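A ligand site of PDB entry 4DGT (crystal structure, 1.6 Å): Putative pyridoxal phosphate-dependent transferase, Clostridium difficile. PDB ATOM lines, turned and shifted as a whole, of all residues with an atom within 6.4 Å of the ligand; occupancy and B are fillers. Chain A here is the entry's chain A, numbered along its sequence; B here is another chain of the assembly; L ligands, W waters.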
ATOM      1  N   ALA A  40      18.484  -9.497   1.368  1.00  0.00           N
ATOM      2  CA  ALA A  40      18.654  -9.987  -0.025  1.00  0.00           C
ATOM      3  C   ALA A  40      17.355 -10.045  -0.808  1.00  0.00           C
ATOM      4  O   ALA A  40      16.760 -11.107  -1.038  1.00  0.00           O
ATOM      5  CB  ALA A  40      19.342 -11.346  -0.076  1.00  0.00           C
ATOM      6  N   PRO A  97       6.618 -23.034   0.894  1.00  0.00           N
ATOM      7  CA  PRO A  97       6.551 -21.582   0.817  1.00  0.00           C
ATOM      8  C   PRO A  97       7.905 -20.906   0.909  1.00  0.00           C
ATOM      9  O   PRO A  97       8.056 -19.777   0.480  1.00  0.00           O
ATOM     10  CB  PRO A  97       5.667 -21.187   1.995  1.00  0.00           C
ATOM     11  CG  PRO A  97       5.609 -22.350   2.831  1.00  0.00           C
ATOM     12  CD  PRO A  97       5.905 -23.570   2.068  1.00  0.00           C
ATOM     13  N   GLY A  98       8.890 -21.626   1.448  1.00  0.00           N
ATOM     14  CA  GLY A  98      10.254 -21.127   1.473  1.00  0.00           C
ATOM     15  C   GLY A  98      11.238 -22.249   1.792  1.00  0.00           C
ATOM     16  O   GLY A  98      10.874 -23.362   2.282  1.00  0.00           O
ATOM     17  N   VAL A  99      12.486 -21.918   1.559  1.00  0.00           N
ATOM     18  CA  VAL A  99      13.585 -22.860   1.826  1.00  0.00           C
ATOM     19  C   VAL A  99      13.683 -23.180   3.307  1.00  0.00           C
ATOM     20  O   VAL A  99      13.805 -24.400   3.634  1.00  0.00           O
ATOM     21  CB  VAL A  99      14.919 -22.311   1.299  1.00  0.00           C
ATOM     22  CG1 VAL A  99      16.133 -23.117   1.849  1.00  0.00           C
ATOM     23  CG2 VAL A  99      14.860 -22.275  -0.214  1.00  0.00           C
ATOM     24  N   ILE A 100      13.725 -22.185   4.197  1.00  0.00           N
ATOM     25  CA  ILE A 100      13.906 -22.496   5.604  1.00  0.00           C
ATOM     26  C   ILE A 100      12.726 -23.280   6.232  1.00  0.00           C
ATOM     27  O   ILE A 100      12.922 -24.236   6.961  1.00  0.00           O
ATOM     28  CB  ILE A 100      14.352 -21.254   6.460  1.00  0.00           C
ATOM     29  CG1 ILE A 100      15.666 -20.664   5.948  1.00  0.00           C
ATOM     30  CG2 ILE A 100      14.405 -21.586   7.962  1.00  0.00           C
ATOM     31  CD1 ILE A 100      16.842 -21.573   6.014  1.00  0.00           C
ATOM     32  N   PRO A 101      11.448 -22.974   5.845  1.00  0.00           N
ATOM     33  CA  PRO A 101      10.385 -23.888   6.246  1.00  0.00           C
ATOM     34  C   PRO A 101      10.632 -25.366   5.904  1.00  0.00           C
ATOM     35  O   PRO A 101      10.401 -26.239   6.703  1.00  0.00           O
ATOM     36  CB  PRO A 101       9.161 -23.332   5.495  1.00  0.00           C
ATOM     37  CG  PRO A 101       9.451 -21.872   5.355  1.00  0.00           C
ATOM     38  CD  PRO A 101      10.916 -21.773   5.192  1.00  0.00           C
ATOM     39  N   VAL A 123      27.752 -18.025   7.717  1.00  0.00           N
ATOM     40  CA  VAL A 123      26.674 -18.414   6.787  1.00  0.00           C
ATOM     41  C   VAL A 123      25.380 -17.759   7.198  1.00  0.00           C
ATOM     42  O   VAL A 123      25.201 -17.402   8.353  1.00  0.00           O
ATOM     43  CB  VAL A 123      26.539 -19.976   6.658  1.00  0.00           C
ATOM     44  CG1 VAL A 123      25.967 -20.577   7.945  1.00  0.00           C
ATOM     45  CG2 VAL A 123      25.770 -20.447   5.380  1.00  0.00           C
ATOM     46  N   TYR A 124      24.478 -17.623   6.220  1.00  0.00           N
ATOM     47  CA  TYR A 124      23.081 -17.253   6.341  1.00  0.00           C
ATOM     48  C   TYR A 124      22.573 -17.678   7.735  1.00  0.00           C
ATOM     49  O   TYR A 124      22.498 -18.867   8.035  1.00  0.00           O
ATOM     50  CB  TYR A 124      22.312 -17.953   5.211  1.00  0.00           C
ATOM     51  CG  TYR A 124      20.829 -17.529   5.111  1.00  0.00           C
ATOM     52  CD1 TYR A 124      20.508 -16.223   4.964  1.00  0.00           C
ATOM     53  CD2 TYR A 124      19.827 -18.490   5.105  1.00  0.00           C
ATOM     54  CE1 TYR A 124      19.170 -15.848   4.841  1.00  0.00           C
ATOM     55  CE2 TYR A 124      18.509 -18.132   4.935  1.00  0.00           C
ATOM     56  CZ  TYR A 124      18.197 -16.810   4.865  1.00  0.00           C
ATOM     57  OH  TYR A 124      16.856 -16.421   4.740  1.00  0.00           O
ATOM     58  N   PHE A 127      20.424 -20.750   9.162  1.00  0.00           N
ATOM     59  CA  PHE A 127      20.985 -22.137   9.280  1.00  0.00           C
ATOM     60  C   PHE A 127      21.250 -22.473  10.757  1.00  0.00           C
ATOM     61  O   PHE A 127      20.980 -23.567  11.176  1.00  0.00           O
ATOM     62  CB  PHE A 127      22.311 -22.304   8.547  1.00  0.00           C
ATOM     63  CG  PHE A 127      22.235 -22.546   7.067  1.00  0.00           C
ATOM     64  CD1 PHE A 127      21.178 -22.158   6.296  1.00  0.00           C
ATOM     65  CD2 PHE A 127      23.317 -23.238   6.474  1.00  0.00           C
ATOM     66  CE1 PHE A 127      21.192 -22.367   4.891  1.00  0.00           C
ATOM     67  CE2 PHE A 127      23.302 -23.483   5.104  1.00  0.00           C
ATOM     68  CZ  PHE A 127      22.261 -23.028   4.341  1.00  0.00           C
ATOM     69  N   CYS A 171      25.484 -24.710   2.007  1.00  0.00           N
ATOM     70  CA  CYS A 171      25.019 -23.481   1.259  1.00  0.00           C
ATOM     71  C   CYS A 171      25.832 -23.419  -0.056  1.00  0.00           C
ATOM     72  O   CYS A 171      27.064 -23.265  -0.026  1.00  0.00           O
ATOM     73  CB  CYS A 171      25.256 -22.248   2.075  1.00  0.00           C
ATOM     74  SG  CYS A 171      24.224 -20.839   1.605  1.00  0.00           S
ATOM     75  N   PRO A 173      25.493 -21.742  -4.022  1.00  0.00           N
ATOM     76  CA  PRO A 173      26.575 -20.876  -3.561  1.00  0.00           C
ATOM     77  C   PRO A 173      26.441 -20.506  -2.117  1.00  0.00           C
ATOM     78  O   PRO A 173      25.326 -20.460  -1.570  1.00  0.00           O
ATOM     79  CB  PRO A 173      26.474 -19.650  -4.424  1.00  0.00           C
ATOM     80  CG  PRO A 173      25.677 -20.090  -5.640  1.00  0.00           C
ATOM     81  CD  PRO A 173      24.740 -21.120  -5.124  1.00  0.00           C
ATOM     82  N   ASN A 175      26.406 -18.065   0.885  1.00  0.00           N
ATOM     83  CA  ASN A 175      26.069 -16.700   1.353  1.00  0.00           C
ATOM     84  C   ASN A 175      26.578 -16.653   2.791  1.00  0.00           C
ATOM     85  O   ASN A 175      26.121 -17.479   3.613  1.00  0.00           O
ATOM     86  CB  ASN A 175      24.523 -16.521   1.317  1.00  0.00           C
ATOM     87  CG  ASN A 175      24.039 -15.344   2.098  1.00  0.00           C
ATOM     88  OD1 ASN A 175      24.775 -14.471   2.552  1.00  0.00           O
ATOM     89  ND2 ASN A 175      22.658 -15.310   2.273  1.00  0.00           N
ATOM     90  N   ASP A 203      21.212 -26.180   0.269  1.00  0.00           N
ATOM     91  CA  ASP A 203      20.440 -24.948   0.005  1.00  0.00           C
ATOM     92  C   ASP A 203      21.071 -24.251  -1.184  1.00  0.00           C
ATOM     93  O   ASP A 203      22.176 -23.680  -1.050  1.00  0.00           O
ATOM     94  CB  ASP A 203      20.463 -24.062   1.253  1.00  0.00           C
ATOM     95  CG  ASP A 203      19.720 -22.750   1.045  1.00  0.00           C
ATOM     96  OD1 ASP A 203      19.363 -22.370  -0.098  1.00  0.00           O
ATOM     97  OD2 ASP A 203      19.491 -22.095   2.086  1.00  0.00           O
ATOM     98  N   ILE A 205      19.583 -21.983  -3.187  1.00  0.00           N
ATOM     99  CA  ILE A 205      18.665 -20.878  -3.609  1.00  0.00           C
ATOM    100  C   ILE A 205      19.378 -19.859  -4.538  1.00  0.00           C
ATOM    101  O   ILE A 205      18.769 -19.277  -5.428  1.00  0.00           O
ATOM    102  CB  ILE A 205      17.974 -20.227  -2.397  1.00  0.00           C
ATOM    103  CG1 ILE A 205      16.740 -19.430  -2.867  1.00  0.00           C
ATOM    104  CG2 ILE A 205      18.928 -19.336  -1.670  1.00  0.00           C
ATOM    105  CD1 ILE A 205      15.918 -18.864  -1.706  1.00  0.00           C
ATOM    106  N   HIS A 206      20.703 -19.673  -4.381  1.00  0.00           N
ATOM    107  CA  HIS A 206      21.459 -18.728  -5.171  1.00  0.00           C
ATOM    108  C   HIS A 206      22.003 -19.354  -6.459  1.00  0.00           C
ATOM    109  O   HIS A 206      22.826 -18.762  -7.131  1.00  0.00           O
ATOM    110  CB  HIS A 206      22.615 -18.136  -4.384  1.00  0.00           C
ATOM    111  CG  HIS A 206      22.203 -17.299  -3.224  1.00  0.00           C
ATOM    112  ND1 HIS A 206      21.906 -15.955  -3.308  1.00  0.00           N
ATOM    113  CD2 HIS A 206      21.943 -17.686  -1.899  1.00  0.00           C
ATOM    114  CE1 HIS A 206      21.568 -15.511  -2.094  1.00  0.00           C
ATOM    115  NE2 HIS A 206      21.547 -16.567  -1.236  1.00  0.00           N
ATOM    116  N   ALA A 235      14.627 -22.246  -5.561  1.00  0.00           N
ATOM    117  CA  ALA A 235      13.454 -21.362  -5.661  1.00  0.00           C
ATOM    118  C   ALA A 235      13.700 -20.402  -6.755  1.00  0.00           C
ATOM    119  O   ALA A 235      14.831 -20.137  -7.133  1.00  0.00           O
ATOM    120  CB  ALA A 235      13.198 -20.604  -4.339  1.00  0.00           C
ATOM    121  N   THR A 237      12.861 -17.270  -6.249  1.00  0.00           N
ATOM    122  CA  THR A 237      12.702 -16.017  -5.547  1.00  0.00           C
ATOM    123  C   THR A 237      13.930 -15.110  -5.570  1.00  0.00           C
ATOM    124  O   THR A 237      13.824 -13.919  -5.846  1.00  0.00           O
ATOM    125  CB  THR A 237      12.226 -16.264  -4.126  1.00  0.00           C
ATOM    126  OG1 THR A 237      13.151 -17.142  -3.440  1.00  0.00           O
ATOM    127  CG2 THR A 237      10.895 -16.870  -4.181  1.00  0.00           C
ATOM    128  N   LYS A 238      15.115 -15.687  -5.278  1.00  0.00           N
ATOM    129  CA  LYS A 238      16.358 -14.873  -5.315  1.00  0.00           C
ATOM    130  C   LYS A 238      16.702 -14.464  -6.746  1.00  0.00           C
ATOM    131  O   LYS A 238      17.003 -13.332  -7.038  1.00  0.00           O
ATOM    132  CB  LYS A 238      17.572 -15.575  -4.654  1.00  0.00           C
ATOM    133  CG  LYS A 238      17.454 -15.756  -3.157  1.00  0.00           C
ATOM    134  CD  LYS A 238      17.859 -14.501  -2.409  1.00  0.00           C
ATOM    135  CE  LYS A 238      17.222 -14.400  -1.036  1.00  0.00           C
ATOM    136  NZ  LYS A 238      18.035 -15.131  -0.098  1.00  0.00           N
ATOM    137  N   ALA A 243      10.571 -12.897  -3.933  1.00  0.00           N
ATOM    138  CA  ALA A 243      10.351 -13.402  -2.543  1.00  0.00           C
ATOM    139  C   ALA A 243       9.027 -13.072  -1.973  1.00  0.00           C
ATOM    140  O   ALA A 243       8.480 -13.905  -1.178  1.00  0.00           O
ATOM    141  CB  ALA A 243      11.514 -12.962  -1.628  1.00  0.00           C
ATOM    142  N   SER A 247       7.601 -18.841  -3.022  1.00  0.00           N
ATOM    143  CA  SER A 247       7.573 -20.081  -3.795  1.00  0.00           C
ATOM    144  C   SER A 247       8.914 -20.698  -3.670  1.00  0.00           C
ATOM    145  O   SER A 247       9.895 -20.034  -3.885  1.00  0.00           O
ATOM    146  CB  SER A 247       7.335 -19.749  -5.286  1.00  0.00           C
ATOM    147  OG  SER A 247       7.551 -20.872  -6.115  1.00  0.00           O
ATOM    148  N   SER A 248       8.995 -21.979  -3.325  1.00  0.00           N
ATOM    149  CA  SER A 248      10.233 -22.714  -3.394  1.00  0.00           C
ATOM    150  C   SER A 248       9.893 -24.190  -3.636  1.00  0.00           C
ATOM    151  O   SER A 248       8.706 -24.585  -3.624  1.00  0.00           O
ATOM    152  CB  SER A 248      11.091 -22.570  -2.133  1.00  0.00           C
ATOM    153  OG  SER A 248      10.498 -23.264  -1.035  1.00  0.00           O
ATOM    154  N   LEU A 327      25.853 -10.479  -3.431  1.00  0.00           N
ATOM    155  CA  LEU A 327      26.216  -9.933  -2.124  1.00  0.00           C
ATOM    156  C   LEU A 327      27.690  -9.843  -2.030  1.00  0.00           C
ATOM    157  O   LEU A 327      28.418 -10.800  -2.409  1.00  0.00           O
ATOM    158  CB  LEU A 327      25.667 -10.928  -1.086  1.00  0.00           C
ATOM    159  CG  LEU A 327      24.196 -11.261  -1.178  1.00  0.00           C
ATOM    160  CD1 LEU A 327      23.759 -12.518  -0.393  1.00  0.00           C
ATOM    161  CD2 LEU A 327      23.380 -10.028  -0.798  1.00  0.00           C
ATOM    162  N   ARG A 369      28.196  -7.172   4.940  1.00  0.00           N
ATOM    163  CA  ARG A 369      27.682  -7.698   3.661  1.00  0.00           C
ATOM    164  C   ARG A 369      26.873  -6.568   2.994  1.00  0.00           C
ATOM    165  O   ARG A 369      25.979  -5.970   3.632  1.00  0.00           O
ATOM    166  CB  ARG A 369      26.783  -8.882   3.879  1.00  0.00           C
ATOM    167  CG  ARG A 369      26.547  -9.666   2.614  1.00  0.00           C
ATOM    168  CD  ARG A 369      25.473 -10.702   2.814  1.00  0.00           C
ATOM    169  NE  ARG A 369      24.161 -10.094   2.911  1.00  0.00           N
ATOM    170  CZ  ARG A 369      23.075 -10.764   3.198  1.00  0.00           C
ATOM    171  NH1 ARG A 369      23.087 -12.079   3.352  1.00  0.00           N
ATOM    172  NH2 ARG A 369      21.925 -10.105   3.254  1.00  0.00           N
ATOM    173  N   TYR B  65      10.497  -8.925  -0.377  1.00  0.00           N
ATOM    174  CA  TYR B  65       9.973  -9.232   0.999  1.00  0.00           C
ATOM    175  C   TYR B  65       9.052  -8.164   1.509  1.00  0.00           C
ATOM    176  O   TYR B  65       9.384  -6.975   1.467  1.00  0.00           O
ATOM    177  CB  TYR B  65      11.162  -9.364   1.960  1.00  0.00           C
ATOM    178  CG  TYR B  65      12.010 -10.576   1.745  1.00  0.00           C
ATOM    179  CD1 TYR B  65      11.558 -11.840   2.049  1.00  0.00           C
ATOM    180  CD2 TYR B  65      13.298 -10.439   1.248  1.00  0.00           C
ATOM    181  CE1 TYR B  65      12.368 -12.946   1.882  1.00  0.00           C
ATOM    182  CE2 TYR B  65      14.095 -11.547   1.069  1.00  0.00           C
ATOM    183  CZ  TYR B  65      13.633 -12.779   1.349  1.00  0.00           C
ATOM    184  OH  TYR B  65      14.493 -13.864   1.181  1.00  0.00           O
ATOM    185  N   ASP B 269       9.834 -20.743  10.283  1.00  0.00           N
ATOM    186  CA  ASP B 269      10.151 -19.539   9.536  1.00  0.00           C
ATOM    187  C   ASP B 269       9.043 -19.133   8.584  1.00  0.00           C
ATOM    188  O   ASP B 269       9.278 -18.841   7.403  1.00  0.00           O
ATOM    189  CB  ASP B 269      11.484 -19.648   8.809  1.00  0.00           C
ATOM    190  CG  ASP B 269      11.964 -18.309   8.289  1.00  0.00           C
ATOM    191  OD1 ASP B 269      11.682 -17.253   8.967  1.00  0.00           O
ATOM    192  OD2 ASP B 269      12.513 -18.333   7.157  1.00  0.00           O
HETATM  193  N1  LIG L   1      18.779 -19.616   1.908  1.00  0.00           N
HETATM  194  C1  LIG L   1      19.737 -18.714   1.654  1.00  0.00           C
HETATM  195  C2  LIG L   1      21.210 -19.129   1.644  1.00  0.00           C
HETATM  196  C3  LIG L   1      19.480 -17.330   1.348  1.00  0.00           C
HETATM  197  O1  LIG L   1      20.446 -16.362   1.185  1.00  0.00           O
HETATM  198  C4  LIG L   1      18.098 -16.923   1.386  1.00  0.00           C
HETATM  199  C5  LIG L   1      17.734 -15.506   1.118  1.00  0.00           C
HETATM  200  C6  LIG L   1      17.079 -17.958   1.674  1.00  0.00           C
HETATM  201  C7  LIG L   1      17.473 -19.276   1.892  1.00  0.00           C
HETATM  202  C8  LIG L   1      15.612 -17.574   1.657  1.00  0.00           C
HETATM  203  O2  LIG L   1      14.984 -18.509   2.464  1.00  0.00           O
HETATM  204  P1  LIG L   1      13.309 -18.552   2.372  1.00  0.00           P
HETATM  205  O3  LIG L   1      13.030 -19.198   1.034  1.00  0.00           O
HETATM  206  O4  LIG L   1      12.941 -19.410   3.631  1.00  0.00           O
HETATM  207  O5  LIG L   1      12.881 -17.067   2.354  1.00  0.00           O
HETATM  208  O   HOH W   1      20.372 -13.697   2.166  1.00  0.00           O
HETATM  209  O   HOH W   2      12.144 -18.816  -1.526  1.00  0.00           O
HETATM  210  O   HOH W   3      10.247 -18.560   4.702  1.00  0.00           O
HETATM  211  O   HOH W   4      16.257 -13.742   3.551  1.00  0.00           O
HETATM  212  O   HOH W   5      12.960 -15.806   0.093  1.00  0.00           O
HETATM  213  O   HOH W   6      14.534 -17.471   5.551  1.00  0.00           O
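A carbon (C5) of the ligand is bonded to the side-chain amino group (NZ) of Lys 238, 1.3 Å away.
OD2 of Asp 203 lies within hydrogen-bond range of N1 of the ligand, at 2.6 Å.
A ring nitrogen (NE2) of His 206 sits at hydrogen-bond distance from an oxygen (O1) of the ligand (2.7 Å).
The side-chain amide nitrogen (ND2) of Asn 175 lies within hydrogen-bond range of an oxygen (O1) of the ligand (2.7 Å).
The backbone NH (N) of Val 99 sits at hydrogen-bond distance from an oxygen (O3) of the ligand, at 2.8 Å.
N of Ile 100 is in hydrogen-bond range of O4 of the ligand, 2.9 Å away.
OD1 of Asp 203 sits at hydrogen-bond distance from N of Ile 205, at 3.1 Å.
N of Tyr 124 lies within hydrogen-bond range of O of Asn 175 (3.1 Å).
The side-chain sulfur of Cys 171 is in hydrogen-bond range of the backbone NH of Asn 175 (3.6 Å).
The side-chain amide oxygen (OD1) of Asn 175 is in hydrogen-bond range of the guanidinium group (NH1) of Arg 369.
The side-chain hydroxyl of Ser 248 sits close to the backbone carbonyl oxygen of Gly 98 (3.3 Å).
The side-chain sulfur of Cys 171 sits close to the backbone carbonyl oxygen of Pro 173.
Merely in contact with the ligand: Tyr 124 (3.4 Å), Gly 98 (3.4 Å), Cys 171 (3.5 Å), Ile 205 (3.5 Å), Pro 101 (3.5 Å), Tyr 65 of chain B (3.6 Å) and Asp 269 of chain B (3.7 Å).
Hydrophobic or aromatic side chains within 4 Å of the ligand: Val 99, Ile 100, Pro 101, Tyr 124, Ile 205 and His 206.
Of the 25 residues printed, 13 come within 4 Å of the ligand.
The nearest printed residue that does not touch the ligand is Phe 127 (4.6 Å).
Water W5 bridges O5 of the ligand (2.6 Å) and OH of Tyr 65 of chain B (2.7 Å).
Water W2 lies within hydrogen-bond range of the side-chain hydroxyl of Thr 237, an oxygen (O3) of the ligand and the backbone carbonyl oxygen of Ser 247.
Water W1 lies within hydrogen-bond range of the side-chain amide nitrogen (ND2) of Asn 175 (2.8 Å), an oxygen (O1) of the ligand (2.8 Å) and the guanidinium group (NH1) of Arg 369 (3.4 Å).
Water W3 lies within hydrogen-bond range of the backbone carbonyl oxygen of Asp 269 of chain B (2.9 Å) and an oxygen (O4) of the ligand (3.0 Å).
Water W6 lies within hydrogen-bond range of OH of Tyr 124 (2.7 Å), OD2 of Asp 269 of chain B (2.7 Å) and O4 of the ligand (3.2 Å).
Water W4 bridges the side-chain hydroxyl of Tyr 65 of chain B (3.0 Å) and the side-chain hydroxyl of Tyr 124 (3.0 Å).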
